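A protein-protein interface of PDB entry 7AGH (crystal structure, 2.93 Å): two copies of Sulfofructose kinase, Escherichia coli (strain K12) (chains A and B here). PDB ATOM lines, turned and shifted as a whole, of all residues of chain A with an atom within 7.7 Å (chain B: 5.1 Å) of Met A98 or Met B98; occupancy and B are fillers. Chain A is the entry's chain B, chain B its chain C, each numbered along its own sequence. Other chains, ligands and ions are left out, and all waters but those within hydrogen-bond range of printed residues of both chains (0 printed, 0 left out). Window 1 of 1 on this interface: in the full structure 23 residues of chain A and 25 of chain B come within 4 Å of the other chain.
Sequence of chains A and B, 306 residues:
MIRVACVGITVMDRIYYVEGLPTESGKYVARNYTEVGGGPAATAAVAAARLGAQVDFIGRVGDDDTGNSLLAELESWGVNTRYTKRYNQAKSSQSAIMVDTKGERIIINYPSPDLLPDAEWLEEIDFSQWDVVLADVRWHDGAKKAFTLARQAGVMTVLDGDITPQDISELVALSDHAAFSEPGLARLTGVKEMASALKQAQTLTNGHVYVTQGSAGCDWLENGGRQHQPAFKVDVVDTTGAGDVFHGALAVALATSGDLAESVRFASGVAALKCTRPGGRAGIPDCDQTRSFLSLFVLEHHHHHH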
ATOM      1  N   ARG A  14     -27.003 -23.701  10.213  1.00  0.00           N
ATOM      2  CA  ARG A  14     -26.999 -22.236  10.409  1.00  0.00           C
ATOM      3  C   ARG A  14     -26.183 -21.976  11.676  1.00  0.00           C
ATOM      4  O   ARG A  14     -26.632 -22.372  12.755  1.00  0.00           O
ATOM      5  CB  ARG A  14     -28.428 -21.694  10.448  1.00  0.00           C
ATOM      6  CG  ARG A  14     -29.191 -21.876   9.145  1.00  0.00           C
ATOM      7  CD  ARG A  14     -30.372 -20.938   8.938  1.00  0.00           C
ATOM      8  NE  ARG A  14     -30.736 -20.812   7.528  1.00  0.00           N
ATOM      9  CZ  ARG A  14     -31.387 -21.738   6.813  1.00  0.00           C
ATOM     10  NH1 ARG A  14     -31.755 -22.886   7.370  1.00  0.00           N
ATOM     11  NH2 ARG A  14     -31.649 -21.511   5.532  1.00  0.00           N
ATOM     12  N   ILE A  15     -25.012 -21.352  11.527  1.00  0.00           N
ATOM     13  CA  ILE A  15     -23.984 -21.161  12.599  1.00  0.00           C
ATOM     14  C   ILE A  15     -23.993 -19.704  13.066  1.00  0.00           C
ATOM     15  O   ILE A  15     -23.708 -18.814  12.247  1.00  0.00           O
ATOM     16  CB  ILE A  15     -22.606 -21.603  12.093  1.00  0.00           C
ATOM     17  CG1 ILE A  15     -22.666 -23.037  11.556  1.00  0.00           C
ATOM     18  CG2 ILE A  15     -21.574 -21.459  13.193  1.00  0.00           C
ATOM     19  CD1 ILE A  15     -21.415 -23.498  10.852  1.00  0.00           C
ATOM     20  N   TYR A  16     -24.351 -19.485  14.329  1.00  0.00           N
ATOM     21  CA  TYR A  16     -24.415 -18.158  14.990  1.00  0.00           C
ATOM     22  C   TYR A  16     -23.196 -18.034  15.911  1.00  0.00           C
ATOM     23  O   TYR A  16     -23.078 -18.864  16.823  1.00  0.00           O
ATOM     24  CB  TYR A  16     -25.742 -18.018  15.749  1.00  0.00           C
ATOM     25  CG  TYR A  16     -26.971 -18.102  14.880  1.00  0.00           C
ATOM     26  CD1 TYR A  16     -27.468 -19.314  14.425  1.00  0.00           C
ATOM     27  CD2 TYR A  16     -27.634 -16.952  14.483  1.00  0.00           C
ATOM     28  CE1 TYR A  16     -28.588 -19.378  13.611  1.00  0.00           C
ATOM     29  CE2 TYR A  16     -28.765 -17.004  13.686  1.00  0.00           C
ATOM     30  CZ  TYR A  16     -29.239 -18.218  13.242  1.00  0.00           C
ATOM     31  OH  TYR A  16     -30.351 -18.236  12.450  1.00  0.00           O
ATOM     32  N   TYR A  17     -22.316 -17.063  15.658  1.00  0.00           N
ATOM     33  CA  TYR A  17     -21.096 -16.787  16.467  1.00  0.00           C
ATOM     34  C   TYR A  17     -21.440 -15.735  17.524  1.00  0.00           C
ATOM     35  O   TYR A  17     -21.813 -14.588  17.161  1.00  0.00           O
ATOM     36  CB  TYR A  17     -19.938 -16.330  15.572  1.00  0.00           C
ATOM     37  CG  TYR A  17     -19.508 -17.401  14.608  1.00  0.00           C
ATOM     38  CD1 TYR A  17     -20.165 -17.562  13.400  1.00  0.00           C
ATOM     39  CD2 TYR A  17     -18.505 -18.297  14.934  1.00  0.00           C
ATOM     40  CE1 TYR A  17     -19.821 -18.577  12.529  1.00  0.00           C
ATOM     41  CE2 TYR A  17     -18.149 -19.317  14.074  1.00  0.00           C
ATOM     42  CZ  TYR A  17     -18.806 -19.453  12.861  1.00  0.00           C
ATOM     43  OH  TYR A  17     -18.474 -20.442  11.982  1.00  0.00           O
ATOM     44  N   VAL A  18     -21.301 -16.117  18.795  1.00  0.00           N
ATOM     45  CA  VAL A  18     -21.785 -15.334  19.968  1.00  0.00           C
ATOM     46  C   VAL A  18     -20.590 -15.039  20.880  1.00  0.00           C
ATOM     47  O   VAL A  18     -19.498 -15.587  20.607  1.00  0.00           O
ATOM     48  CB  VAL A  18     -22.911 -16.100  20.696  1.00  0.00           C
ATOM     49  CG1 VAL A  18     -24.192 -16.090  19.873  1.00  0.00           C
ATOM     50  CG2 VAL A  18     -22.512 -17.523  21.080  1.00  0.00           C
ATOM     51  N   GLY A  20     -20.619 -15.240  24.511  1.00  0.00           N
ATOM     52  CA  GLY A  20     -20.727 -16.414  25.397  1.00  0.00           C
ATOM     53  C   GLY A  20     -21.861 -17.325  24.965  1.00  0.00           C
ATOM     54  O   GLY A  20     -22.826 -16.833  24.362  1.00  0.00           O
ATOM     55  N   LEU A  21     -21.777 -18.616  25.282  1.00  0.00           N
ATOM     56  CA  LEU A  21     -22.904 -19.570  25.112  1.00  0.00           C
ATOM     57  C   LEU A  21     -24.021 -19.149  26.062  1.00  0.00           C
ATOM     58  O   LEU A  21     -23.760 -18.798  27.203  1.00  0.00           O
ATOM     59  CB  LEU A  21     -22.453 -21.009  25.389  1.00  0.00           C
ATOM     60  CG  LEU A  21     -21.539 -21.634  24.334  1.00  0.00           C
ATOM     61  CD1 LEU A  21     -21.295 -23.103  24.643  1.00  0.00           C
ATOM     62  CD2 LEU A  21     -22.074 -21.476  22.910  1.00  0.00           C
ATOM     63  N   PRO A  22     -25.295 -19.162  25.603  1.00  0.00           N
ATOM     64  CA  PRO A  22     -26.455 -18.906  26.456  1.00  0.00           C
ATOM     65  C   PRO A  22     -26.512 -19.736  27.751  1.00  0.00           C
ATOM     66  O   PRO A  22     -26.637 -20.940  27.705  1.00  0.00           O
ATOM     67  CB  PRO A  22     -27.656 -19.270  25.562  1.00  0.00           C
ATOM     68  CG  PRO A  22     -27.069 -20.071  24.440  1.00  0.00           C
ATOM     69  CD  PRO A  22     -25.704 -19.446  24.222  1.00  0.00           C
ATOM     70  N   SER A  25     -32.380 -18.224  29.981  1.00  0.00           N
ATOM     71  CA  SER A  25     -33.404 -17.605  29.094  1.00  0.00           C
ATOM     72  C   SER A  25     -33.043 -16.145  28.771  1.00  0.00           C
ATOM     73  O   SER A  25     -32.308 -15.540  29.569  1.00  0.00           O
ATOM     74  CB  SER A  25     -34.768 -17.710  29.746  1.00  0.00           C
ATOM     75  OG  SER A  25     -35.727 -16.885  29.121  1.00  0.00           O
ATOM     76  N   GLY A  26     -33.509 -15.620  27.630  1.00  0.00           N
ATOM     77  CA  GLY A  26     -33.330 -14.213  27.218  1.00  0.00           C
ATOM     78  C   GLY A  26     -32.830 -14.052  25.786  1.00  0.00           C
ATOM     79  O   GLY A  26     -32.546 -15.069  25.127  1.00  0.00           O
ATOM     80  N   TYR A  28     -30.072 -12.764  22.978  1.00  0.00           N
ATOM     81  CA  TYR A  28     -28.617 -12.653  22.712  1.00  0.00           C
ATOM     82  C   TYR A  28     -28.405 -12.194  21.271  1.00  0.00           C
ATOM     83  O   TYR A  28     -29.292 -12.427  20.430  1.00  0.00           O
ATOM     84  CB  TYR A  28     -27.929 -14.004  22.882  1.00  0.00           C
ATOM     85  CG  TYR A  28     -28.073 -14.610  24.250  1.00  0.00           C
ATOM     86  CD1 TYR A  28     -29.272 -15.180  24.653  1.00  0.00           C
ATOM     87  CD2 TYR A  28     -27.008 -14.618  25.141  1.00  0.00           C
ATOM     88  CE1 TYR A  28     -29.412 -15.751  25.908  1.00  0.00           C
ATOM     89  CE2 TYR A  28     -27.130 -15.178  26.402  1.00  0.00           C
ATOM     90  CZ  TYR A  28     -28.335 -15.749  26.783  1.00  0.00           C
ATOM     91  OH  TYR A  28     -28.465 -16.289  28.028  1.00  0.00           O
ATOM     92  N   ALA A  30     -25.765 -12.236  17.877  1.00  0.00           N
ATOM     93  CA  ALA A  30     -24.669 -12.934  17.173  1.00  0.00           C
ATOM     94  C   ALA A  30     -23.785 -11.887  16.490  1.00  0.00           C
ATOM     95  O   ALA A  30     -24.306 -11.113  15.672  1.00  0.00           O
ATOM     96  CB  ALA A  30     -25.226 -13.925  16.178  1.00  0.00           C
ATOM     97  N   SER A  95     -29.884 -27.683  11.233  1.00  0.00           N
ATOM     98  CA  SER A  95     -29.341 -27.497  12.606  1.00  0.00           C
ATOM     99  C   SER A  95     -29.031 -26.019  12.842  1.00  0.00           C
ATOM    100  O   SER A  95     -28.558 -25.356  11.914  1.00  0.00           O
ATOM    101  CB  SER A  95     -28.135 -28.349  12.844  1.00  0.00           C
ATOM    102  OG  SER A  95     -28.498 -29.718  12.956  1.00  0.00           O
ATOM    103  N   ALA A  96     -29.378 -25.505  14.018  1.00  0.00           N
ATOM    104  CA  ALA A  96     -28.896 -24.209  14.526  1.00  0.00           C
ATOM    105  C   ALA A  96     -27.707 -24.513  15.432  1.00  0.00           C
ATOM    106  O   ALA A  96     -27.851 -25.327  16.331  1.00  0.00           O
ATOM    107  CB  ALA A  96     -29.992 -23.452  15.234  1.00  0.00           C
ATOM    108  N   ILE A  97     -26.566 -23.884  15.171  1.00  0.00           N
ATOM    109  CA  ILE A  97     -25.314 -24.048  15.963  1.00  0.00           C
ATOM    110  C   ILE A  97     -24.905 -22.693  16.555  1.00  0.00           C
ATOM    111  O   ILE A  97     -24.747 -21.724  15.781  1.00  0.00           O
ATOM    112  CB  ILE A  97     -24.224 -24.681  15.076  1.00  0.00           C
ATOM    113  CG1 ILE A  97     -24.712 -25.999  14.470  1.00  0.00           C
ATOM    114  CG2 ILE A  97     -22.935 -24.865  15.866  1.00  0.00           C
ATOM    115  CD1 ILE A  97     -23.765 -26.629  13.488  1.00  0.00           C
ATOM    116  N   MET A  98     -24.750 -22.632  17.879  1.00  0.00           N
ATOM    117  CA  MET A  98     -24.130 -21.481  18.600  1.00  0.00           C
ATOM    118  C   MET A  98     -22.652 -21.780  18.850  1.00  0.00           C
ATOM    119  O   MET A  98     -22.371 -22.868  19.380  1.00  0.00           O
ATOM    120  CB  MET A  98     -24.794 -21.238  19.957  1.00  0.00           C
ATOM    121  CG  MET A  98     -26.066 -20.474  19.894  1.00  0.00           C
ATOM    122  SD  MET A  98     -27.248 -21.355  20.896  1.00  0.00           S
ATOM    123  CE  MET A  98     -27.842 -22.508  19.654  1.00  0.00           C
ATOM    124  N   VAL A  99     -21.761 -20.849  18.497  1.00  0.00           N
ATOM    125  CA  VAL A  99     -20.294 -20.953  18.769  1.00  0.00           C
ATOM    126  C   VAL A  99     -19.846 -19.747  19.599  1.00  0.00           C
ATOM    127  O   VAL A  99     -20.064 -18.611  19.146  1.00  0.00           O
ATOM    128  CB  VAL A  99     -19.485 -21.045  17.467  1.00  0.00           C
ATOM    129  CG1 VAL A  99     -18.034 -21.400  17.750  1.00  0.00           C
ATOM    130  CG2 VAL A  99     -20.103 -22.035  16.480  1.00  0.00           C
ATOM    131  N   ASP A 100     -19.264 -19.982  20.781  1.00  0.00           N
ATOM    132  CA  ASP A 100     -18.684 -18.876  21.600  1.00  0.00           C
ATOM    133  C   ASP A 100     -17.248 -18.622  21.123  1.00  0.00           C
ATOM    134  O   ASP A 100     -16.808 -19.285  20.173  1.00  0.00           O
ATOM    135  CB  ASP A 100     -18.848 -19.054  23.117  1.00  0.00           C
ATOM    136  CG  ASP A 100     -18.048 -20.169  23.759  1.00  0.00           C
ATOM    137  OD1 ASP A 100     -17.076 -20.657  23.114  1.00  0.00           O
ATOM    138  OD2 ASP A 100     -18.394 -20.518  24.914  1.00  0.00           O
ATOM    139  N   GLY A 103     -14.758 -21.418  21.217  1.00  0.00           N
ATOM    140  CA  GLY A 103     -15.086 -22.404  20.172  1.00  0.00           C
ATOM    141  C   GLY A 103     -16.037 -23.479  20.685  1.00  0.00           C
ATOM    142  O   GLY A 103     -16.370 -24.387  19.877  1.00  0.00           O
ATOM    143  N   GLU A 104     -16.455 -23.402  21.961  1.00  0.00           N
ATOM    144  CA  GLU A 104     -17.518 -24.267  22.549  1.00  0.00           C
ATOM    145  C   GLU A 104     -18.794 -24.153  21.698  1.00  0.00           C
ATOM    146  O   GLU A 104     -19.154 -23.003  21.320  1.00  0.00           O
ATOM    147  CB  GLU A 104     -17.809 -23.871  23.997  1.00  0.00           C
ATOM    148  N   ARG A 105     -19.432 -25.288  21.379  1.00  0.00           N
ATOM    149  CA  ARG A 105     -20.545 -25.358  20.388  1.00  0.00           C
ATOM    150  C   ARG A 105     -21.801 -25.890  21.092  1.00  0.00           C
ATOM    151  O   ARG A 105     -21.654 -26.752  21.968  1.00  0.00           O
ATOM    152  CB  ARG A 105     -20.126 -26.207  19.180  1.00  0.00           C
ATOM    153  N   ILE A 106     -22.976 -25.329  20.787  1.00  0.00           N
ATOM    154  CA  ILE A 106     -24.313 -25.933  21.083  1.00  0.00           C
ATOM    155  C   ILE A 106     -24.974 -26.245  19.741  1.00  0.00           C
ATOM    156  O   ILE A 106     -25.057 -25.332  18.913  1.00  0.00           O
ATOM    157  CB  ILE A 106     -25.196 -24.997  21.936  1.00  0.00           C
ATOM    158  CG1 ILE A 106     -24.705 -24.905  23.382  1.00  0.00           C
ATOM    159  CG2 ILE A 106     -26.661 -25.410  21.872  1.00  0.00           C
ATOM    160  CD1 ILE A 106     -25.441 -23.865  24.204  1.00  0.00           C
ATOM    161  N   ILE A 107     -25.420 -27.482  19.530  1.00  0.00           N
ATOM    162  CA  ILE A 107     -26.086 -27.909  18.265  1.00  0.00           C
ATOM    163  C   ILE A 107     -27.523 -28.305  18.592  1.00  0.00           C
ATOM    164  O   ILE A 107     -27.706 -29.179  19.419  1.00  0.00           O
ATOM    165  CB  ILE A 107     -25.314 -29.062  17.598  1.00  0.00           C
ATOM    166  CG1 ILE A 107     -23.838 -28.714  17.397  1.00  0.00           C
ATOM    167  CG2 ILE A 107     -25.976 -29.467  16.291  1.00  0.00           C
ATOM    168  CD1 ILE A 107     -22.928 -29.920  17.380  1.00  0.00           C
ATOM    169  N   ILE A 108     -28.489 -27.639  17.975  1.00  0.00           N
ATOM    170  CA  ILE A 108     -29.930 -28.000  18.001  1.00  0.00           C
ATOM    171  C   ILE A 108     -30.240 -28.594  16.632  1.00  0.00           C
ATOM    172  O   ILE A 108     -30.289 -27.802  15.659  1.00  0.00           O
ATOM    173  CB  ILE A 108     -30.820 -26.773  18.284  1.00  0.00           C
ATOM    174  CG1 ILE A 108     -30.210 -25.818  19.312  1.00  0.00           C
ATOM    175  CG2 ILE A 108     -32.219 -27.200  18.681  1.00  0.00           C
ATOM    176  CD1 ILE A 108     -30.189 -26.335  20.743  1.00  0.00           C
ATOM    177  N   ASP A 238     -13.592 -22.352  14.898  1.00  0.00           N
ATOM    178  CA  ASP A 238     -14.869 -23.121  14.847  1.00  0.00           C
ATOM    179  C   ASP A 238     -14.540 -24.619  14.788  1.00  0.00           C
ATOM    180  O   ASP A 238     -13.866 -25.059  13.826  1.00  0.00           O
ATOM    181  CB  ASP A 238     -15.745 -22.688  13.652  1.00  0.00           C
ATOM    182  CG  ASP A 238     -17.202 -23.123  13.758  1.00  0.00           C
ATOM    183  OD1 ASP A 238     -17.512 -23.988  14.611  1.00  0.00           O
ATOM    184  OD2 ASP A 238     -18.019 -22.610  12.969  1.00  0.00           O
ATOM    185  N   THR A 240     -17.008 -26.870  14.727  1.00  0.00           N
ATOM    186  CA  THR A 240     -18.197 -27.447  14.049  1.00  0.00           C
ATOM    187  C   THR A 240     -17.714 -28.401  12.961  1.00  0.00           C
ATOM    188  O   THR A 240     -16.910 -27.959  12.124  1.00  0.00           O
ATOM    189  CB  THR A 240     -19.104 -26.352  13.475  1.00  0.00           C
ATOM    190  OG1 THR A 240     -19.552 -25.528  14.551  1.00  0.00           O
ATOM    191  CG2 THR A 240     -20.308 -26.914  12.751  1.00  0.00           C
ATOM    192  N   TYR B  16     -37.170 -23.555  17.350  1.00  0.00           N
ATOM    193  CA  TYR B  16     -36.830 -24.951  17.703  1.00  0.00           C
ATOM    194  C   TYR B  16     -37.469 -25.255  19.062  1.00  0.00           C
ATOM    195  O   TYR B  16     -37.143 -24.550  20.014  1.00  0.00           O
ATOM    196  CB  TYR B  16     -35.311 -25.121  17.741  1.00  0.00           C
ATOM    197  CG  TYR B  16     -34.614 -24.863  16.437  1.00  0.00           C
ATOM    198  CD1 TYR B  16     -34.343 -23.575  16.017  1.00  0.00           C
ATOM    199  CD2 TYR B  16     -34.186 -25.902  15.634  1.00  0.00           C
ATOM    200  CE1 TYR B  16     -33.691 -23.321  14.818  1.00  0.00           C
ATOM    201  CE2 TYR B  16     -33.538 -25.669  14.430  1.00  0.00           C
ATOM    202  CZ  TYR B  16     -33.293 -24.374  14.021  1.00  0.00           C
ATOM    203  OH  TYR B  16     -32.669 -24.108  12.839  1.00  0.00           O
ATOM    204  N   VAL B  18     -37.747 -27.598  22.242  1.00  0.00           N
ATOM    205  CA  VAL B  18     -36.813 -28.507  22.967  1.00  0.00           C
ATOM    206  C   VAL B  18     -37.453 -28.914  24.298  1.00  0.00           C
ATOM    207  O   VAL B  18     -38.509 -28.356  24.641  1.00  0.00           O
ATOM    208  CB  VAL B  18     -35.442 -27.828  23.167  1.00  0.00           C
ATOM    209  CG1 VAL B  18     -34.680 -27.720  21.861  1.00  0.00           C
ATOM    210  CG2 VAL B  18     -35.546 -26.459  23.836  1.00  0.00           C
ATOM    211  N   LEU B  21     -34.025 -25.880  27.964  1.00  0.00           N
ATOM    212  CA  LEU B  21     -33.207 -24.846  27.269  1.00  0.00           C
ATOM    213  C   LEU B  21     -31.741 -25.267  27.287  1.00  0.00           C
ATOM    214  O   LEU B  21     -31.253 -25.733  28.311  1.00  0.00           O
ATOM    215  CB  LEU B  21     -33.411 -23.475  27.932  1.00  0.00           C
ATOM    216  CG  LEU B  21     -34.761 -22.808  27.646  1.00  0.00           C
ATOM    217  CD1 LEU B  21     -34.842 -21.419  28.263  1.00  0.00           C
ATOM    218  CD2 LEU B  21     -34.981 -22.729  26.152  1.00  0.00           C
ATOM    219  N   PRO B  22     -31.022 -25.167  26.145  1.00  0.00           N
ATOM    220  CA  PRO B  22     -29.610 -25.586  26.091  1.00  0.00           C
ATOM    221  C   PRO B  22     -28.671 -24.734  26.968  1.00  0.00           C
ATOM    222  O   PRO B  22     -28.369 -23.609  26.576  1.00  0.00           O
ATOM    223  CB  PRO B  22     -29.270 -25.460  24.598  1.00  0.00           C
ATOM    224  CG  PRO B  22     -30.325 -24.523  24.022  1.00  0.00           C
ATOM    225  CD  PRO B  22     -31.573 -24.735  24.845  1.00  0.00           C
ATOM    226  N   ALA B  96     -32.420 -17.577  15.591  1.00  0.00           N
ATOM    227  CA  ALA B  96     -32.719 -18.938  16.079  1.00  0.00           C
ATOM    228  C   ALA B  96     -33.327 -18.796  17.472  1.00  0.00           C
ATOM    229  O   ALA B  96     -32.717 -18.115  18.321  1.00  0.00           O
ATOM    230  CB  ALA B  96     -31.468 -19.767  16.094  1.00  0.00           C
ATOM    231  N   ILE B  97     -34.517 -19.353  17.673  1.00  0.00           N
ATOM    232  CA  ILE B  97     -35.237 -19.288  18.978  1.00  0.00           C
ATOM    233  C   ILE B  97     -35.450 -20.716  19.472  1.00  0.00           C
ATOM    234  O   ILE B  97     -36.116 -21.503  18.751  1.00  0.00           O
ATOM    235  CB  ILE B  97     -36.551 -18.492  18.844  1.00  0.00           C
ATOM    236  CG1 ILE B  97     -36.303 -17.126  18.186  1.00  0.00           C
ATOM    237  CG2 ILE B  97     -37.264 -18.396  20.187  1.00  0.00           C
ATOM    238  CD1 ILE B  97     -37.557 -16.325  17.937  1.00  0.00           C
ATOM    239  N   MET B  98     -34.888 -21.025  20.646  1.00  0.00           N
ATOM    240  CA  MET B  98     -35.143 -22.276  21.409  1.00  0.00           C
ATOM    241  C   MET B  98     -36.286 -22.028  22.392  1.00  0.00           C
ATOM    242  O   MET B  98     -36.226 -21.043  23.111  1.00  0.00           O
ATOM    243  CB  MET B  98     -33.909 -22.709  22.207  1.00  0.00           C
ATOM    244  CG  MET B  98     -32.919 -23.509  21.398  1.00  0.00           C
ATOM    245  SD  MET B  98     -32.433 -22.625  19.909  1.00  0.00           S
ATOM    246  CE  MET B  98     -31.323 -21.407  20.624  1.00  0.00           C
ATOM    247  N   VAL B  99     -37.285 -22.905  22.404  1.00  0.00           N
ATOM    248  CA  VAL B  99     -38.468 -22.832  23.305  1.00  0.00           C
ATOM    249  C   VAL B  99     -38.536 -24.139  24.095  1.00  0.00           C
ATOM    250  O   VAL B  99     -38.589 -25.209  23.465  1.00  0.00           O
ATOM    251  CB  VAL B  99     -39.762 -22.580  22.508  1.00  0.00           C
ATOM    252  CG1 VAL B  99     -40.942 -22.324  23.437  1.00  0.00           C
ATOM    253  CG2 VAL B  99     -39.588 -21.446  21.496  1.00  0.00           C
ATOM    254  N   ASP B 100     -38.508 -23.985  25.421  1.00  0.00           N
ATOM    255  CA  ASP B 100     -38.725 -24.958  26.513  1.00  0.00           C
ATOM    256  C   ASP B 100     -40.173 -25.449  26.474  1.00  0.00           C
ATOM    257  O   ASP B 100     -41.024 -24.750  25.888  1.00  0.00           O
ATOM    258  CB  ASP B 100     -38.540 -24.209  27.846  1.00  0.00           C
ATOM    259  CG  ASP B 100     -37.698 -24.906  28.896  1.00  0.00           C
ATOM    260  OD1 ASP B 100     -37.636 -26.149  28.862  1.00  0.00           O
ATOM    261  OD2 ASP B 100     -37.075 -24.195  29.720  1.00  0.00           O
ATOM    262  N   GLU B 104     -40.352 -20.710  28.045  1.00  0.00           N
ATOM    263  CA  GLU B 104     -39.086 -19.950  28.198  1.00  0.00           C
ATOM    264  C   GLU B 104     -38.330 -20.004  26.865  1.00  0.00           C
ATOM    265  O   GLU B 104     -38.246 -21.086  26.267  1.00  0.00           O
ATOM    266  CB  GLU B 104     -38.233 -20.526  29.329  1.00  0.00           C
ATOM    267  CG  GLU B 104     -38.896 -20.445  30.695  1.00  0.00           C
ATOM    268  CD  GLU B 104     -38.191 -21.285  31.747  1.00  0.00           C
ATOM    269  OE1 GLU B 104     -38.586 -22.472  31.937  1.00  0.00           O
ATOM    270  OE2 GLU B 104     -37.210 -20.773  32.333  1.00  0.00           O
ATOM    271  N   ARG B 105     -37.800 -18.860  26.425  1.00  0.00           N
ATOM    272  CA  ARG B 105     -37.149 -18.674  25.111  1.00  0.00           C
ATOM    273  C   ARG B 105     -35.659 -18.376  25.349  1.00  0.00           C
ATOM    274  O   ARG B 105     -35.309 -17.721  26.343  1.00  0.00           O
ATOM    275  CB  ARG B 105     -37.838 -17.543  24.350  1.00  0.00           C
ATOM    276  CG  ARG B 105     -39.166 -17.904  23.704  1.00  0.00           C
ATOM    277  CD  ARG B 105     -39.977 -16.665  23.322  1.00  0.00           C
ATOM    278  N   ILE B 106     -34.800 -18.922  24.491  1.00  0.00           N
ATOM    279  CA  ILE B 106     -33.452 -18.365  24.178  1.00  0.00           C
ATOM    280  C   ILE B 106     -33.538 -17.818  22.757  1.00  0.00           C
ATOM    281  O   ILE B 106     -33.904 -18.573  21.847  1.00  0.00           O
ATOM    282  CB  ILE B 106     -32.348 -19.427  24.312  1.00  0.00           C
ATOM    283  CG1 ILE B 106     -32.119 -19.807  25.777  1.00  0.00           C
ATOM    284  CG2 ILE B 106     -31.076 -18.954  23.605  1.00  0.00           C
ATOM    285  CD1 ILE B 106     -30.998 -20.798  25.999  1.00  0.00           C
ATOM    286  N   ILE B 108     -31.285 -16.064  19.798  1.00  0.00           N
ATOM    287  CA  ILE B 108     -29.992 -15.660  19.177  1.00  0.00           C
ATOM    288  C   ILE B 108     -30.358 -14.838  17.948  1.00  0.00           C
ATOM    289  O   ILE B 108     -30.792 -15.453  16.954  1.00  0.00           O
ATOM    290  CB  ILE B 108     -29.128 -16.879  18.798  1.00  0.00           C
ATOM    291  CG1 ILE B 108     -29.221 -18.001  19.835  1.00  0.00           C
ATOM    292  CG2 ILE B 108     -27.693 -16.443  18.544  1.00  0.00           C
ATOM    293  CD1 ILE B 108     -28.490 -17.709  21.144  1.00  0.00           C
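The backbone carbonyl oxygen (O) of Tyr B16 is in hydrogen-bond range of the backbone NH (N) of Val B99 (2.9 Å). O of Ala B96 sits at hydrogen-bond distance from N of Ile B108, at 2.9 Å. The backbone NH (N) of Tyr A16 is in hydrogen-bond range of the backbone carbonyl oxygen (O) of Ile A97, 2.7 Å away. The backbone NH (N) of Val A99 lies within hydrogen-bond range of the backbone carbonyl oxygen (O) of Tyr A16 (2.9 Å). N of Ile A108 sits at hydrogen-bond distance from O of Ala A96, 2.9 Å away. N of Ile A106 sits at hydrogen-bond distance from O of Met A98.
Ala B96 touches Tyr A16. CG2 of Ile B108 touches CB of Tyr A16, 3.8 Å away. Pro A22 touches Ile B106 (CB to CD1, 3.7 Å). Ser A25 touches Leu B21 (CB to CD1, 3.995 Å). Tyr A28 touches Ile B108 (O to CA, 3.5 Å). SD of Met A98 touches CD1 of Ile B108 (3.9 Å). CB of Pro B22 touches CG2 of Ile A106 (3.8 Å). CG2 of Ile A108 touches CB of Tyr B16, 3.8 Å away. Pro B22 touches Ile A108. SD of Met B98 touches CG1 of Ile A108 (3.9 Å).
Printed residues of chain A that touch a printed residue of chain B: Tyr A16, Val A18, Pro A22, Ser A25, Gly A26, Tyr A28, Ala A96, Met A98, Ile A106 and Ile A108. Of the 13 printed residues of chain B, 8 touch a printed residue of chain A. Hydrophobic or aromatic side chains of chain B that line the printed part of chain A: Tyr B16, Leu B21, Pro B22, Ala B96, Met B98, Ile B106 and Ile B108. Among the printed residues, 17 pairs touch across the chains.
O of Arg B105 sits at hydrogen-bond distance from OG of Ser A25. The backbone carbonyl oxygen (O) of Arg B105 lies within hydrogen-bond range of the backbone NH (N) of Gly A26, 3.1 Å away. The backbone carbonyl oxygen (O) of Pro B22 lies close to the backbone carbonyl oxygen (O) of Pro A22, 3.4 Å away.
Tyr A16 touches Ile B108, and with the chains exchanged Ile A108 touches Tyr B16. Pro A22 touches Ile B106, and with the chains exchanged Ile A106 touches Pro B22. Met A98 touches Ile B108, and with the chains exchanged Ile A108 touches Met B98. Ile A108 touches Pro B22, but with the chains exchanged Pro A22 does not touch Ile B108 (4.3 Å). 13 positions are printed for both chains.
Of chain B, only Met B98 and Ile B108 come within 4 Å of Met A98. Arg A105 touches none of the printed residues of chain B. Of the printed residues of chain A, Pro B22 touches Pro A22, Ile A106 and Ile A108. Ile B97 touches none of the printed residues of chain A. Met B98 touches just these residues of chain A: Met A98 and Ile A108. Of the printed residues of chain A, Ile B106 touches Pro A22 (3.7 Å) and Gly A26 (3.5 Å). The nearest residue of chain A that does not touch Met B98 is Ala A96 (5.3 Å). The nearest printed residue of chain A that does not touch Leu B21 is Gly A26 (6.0 Å).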
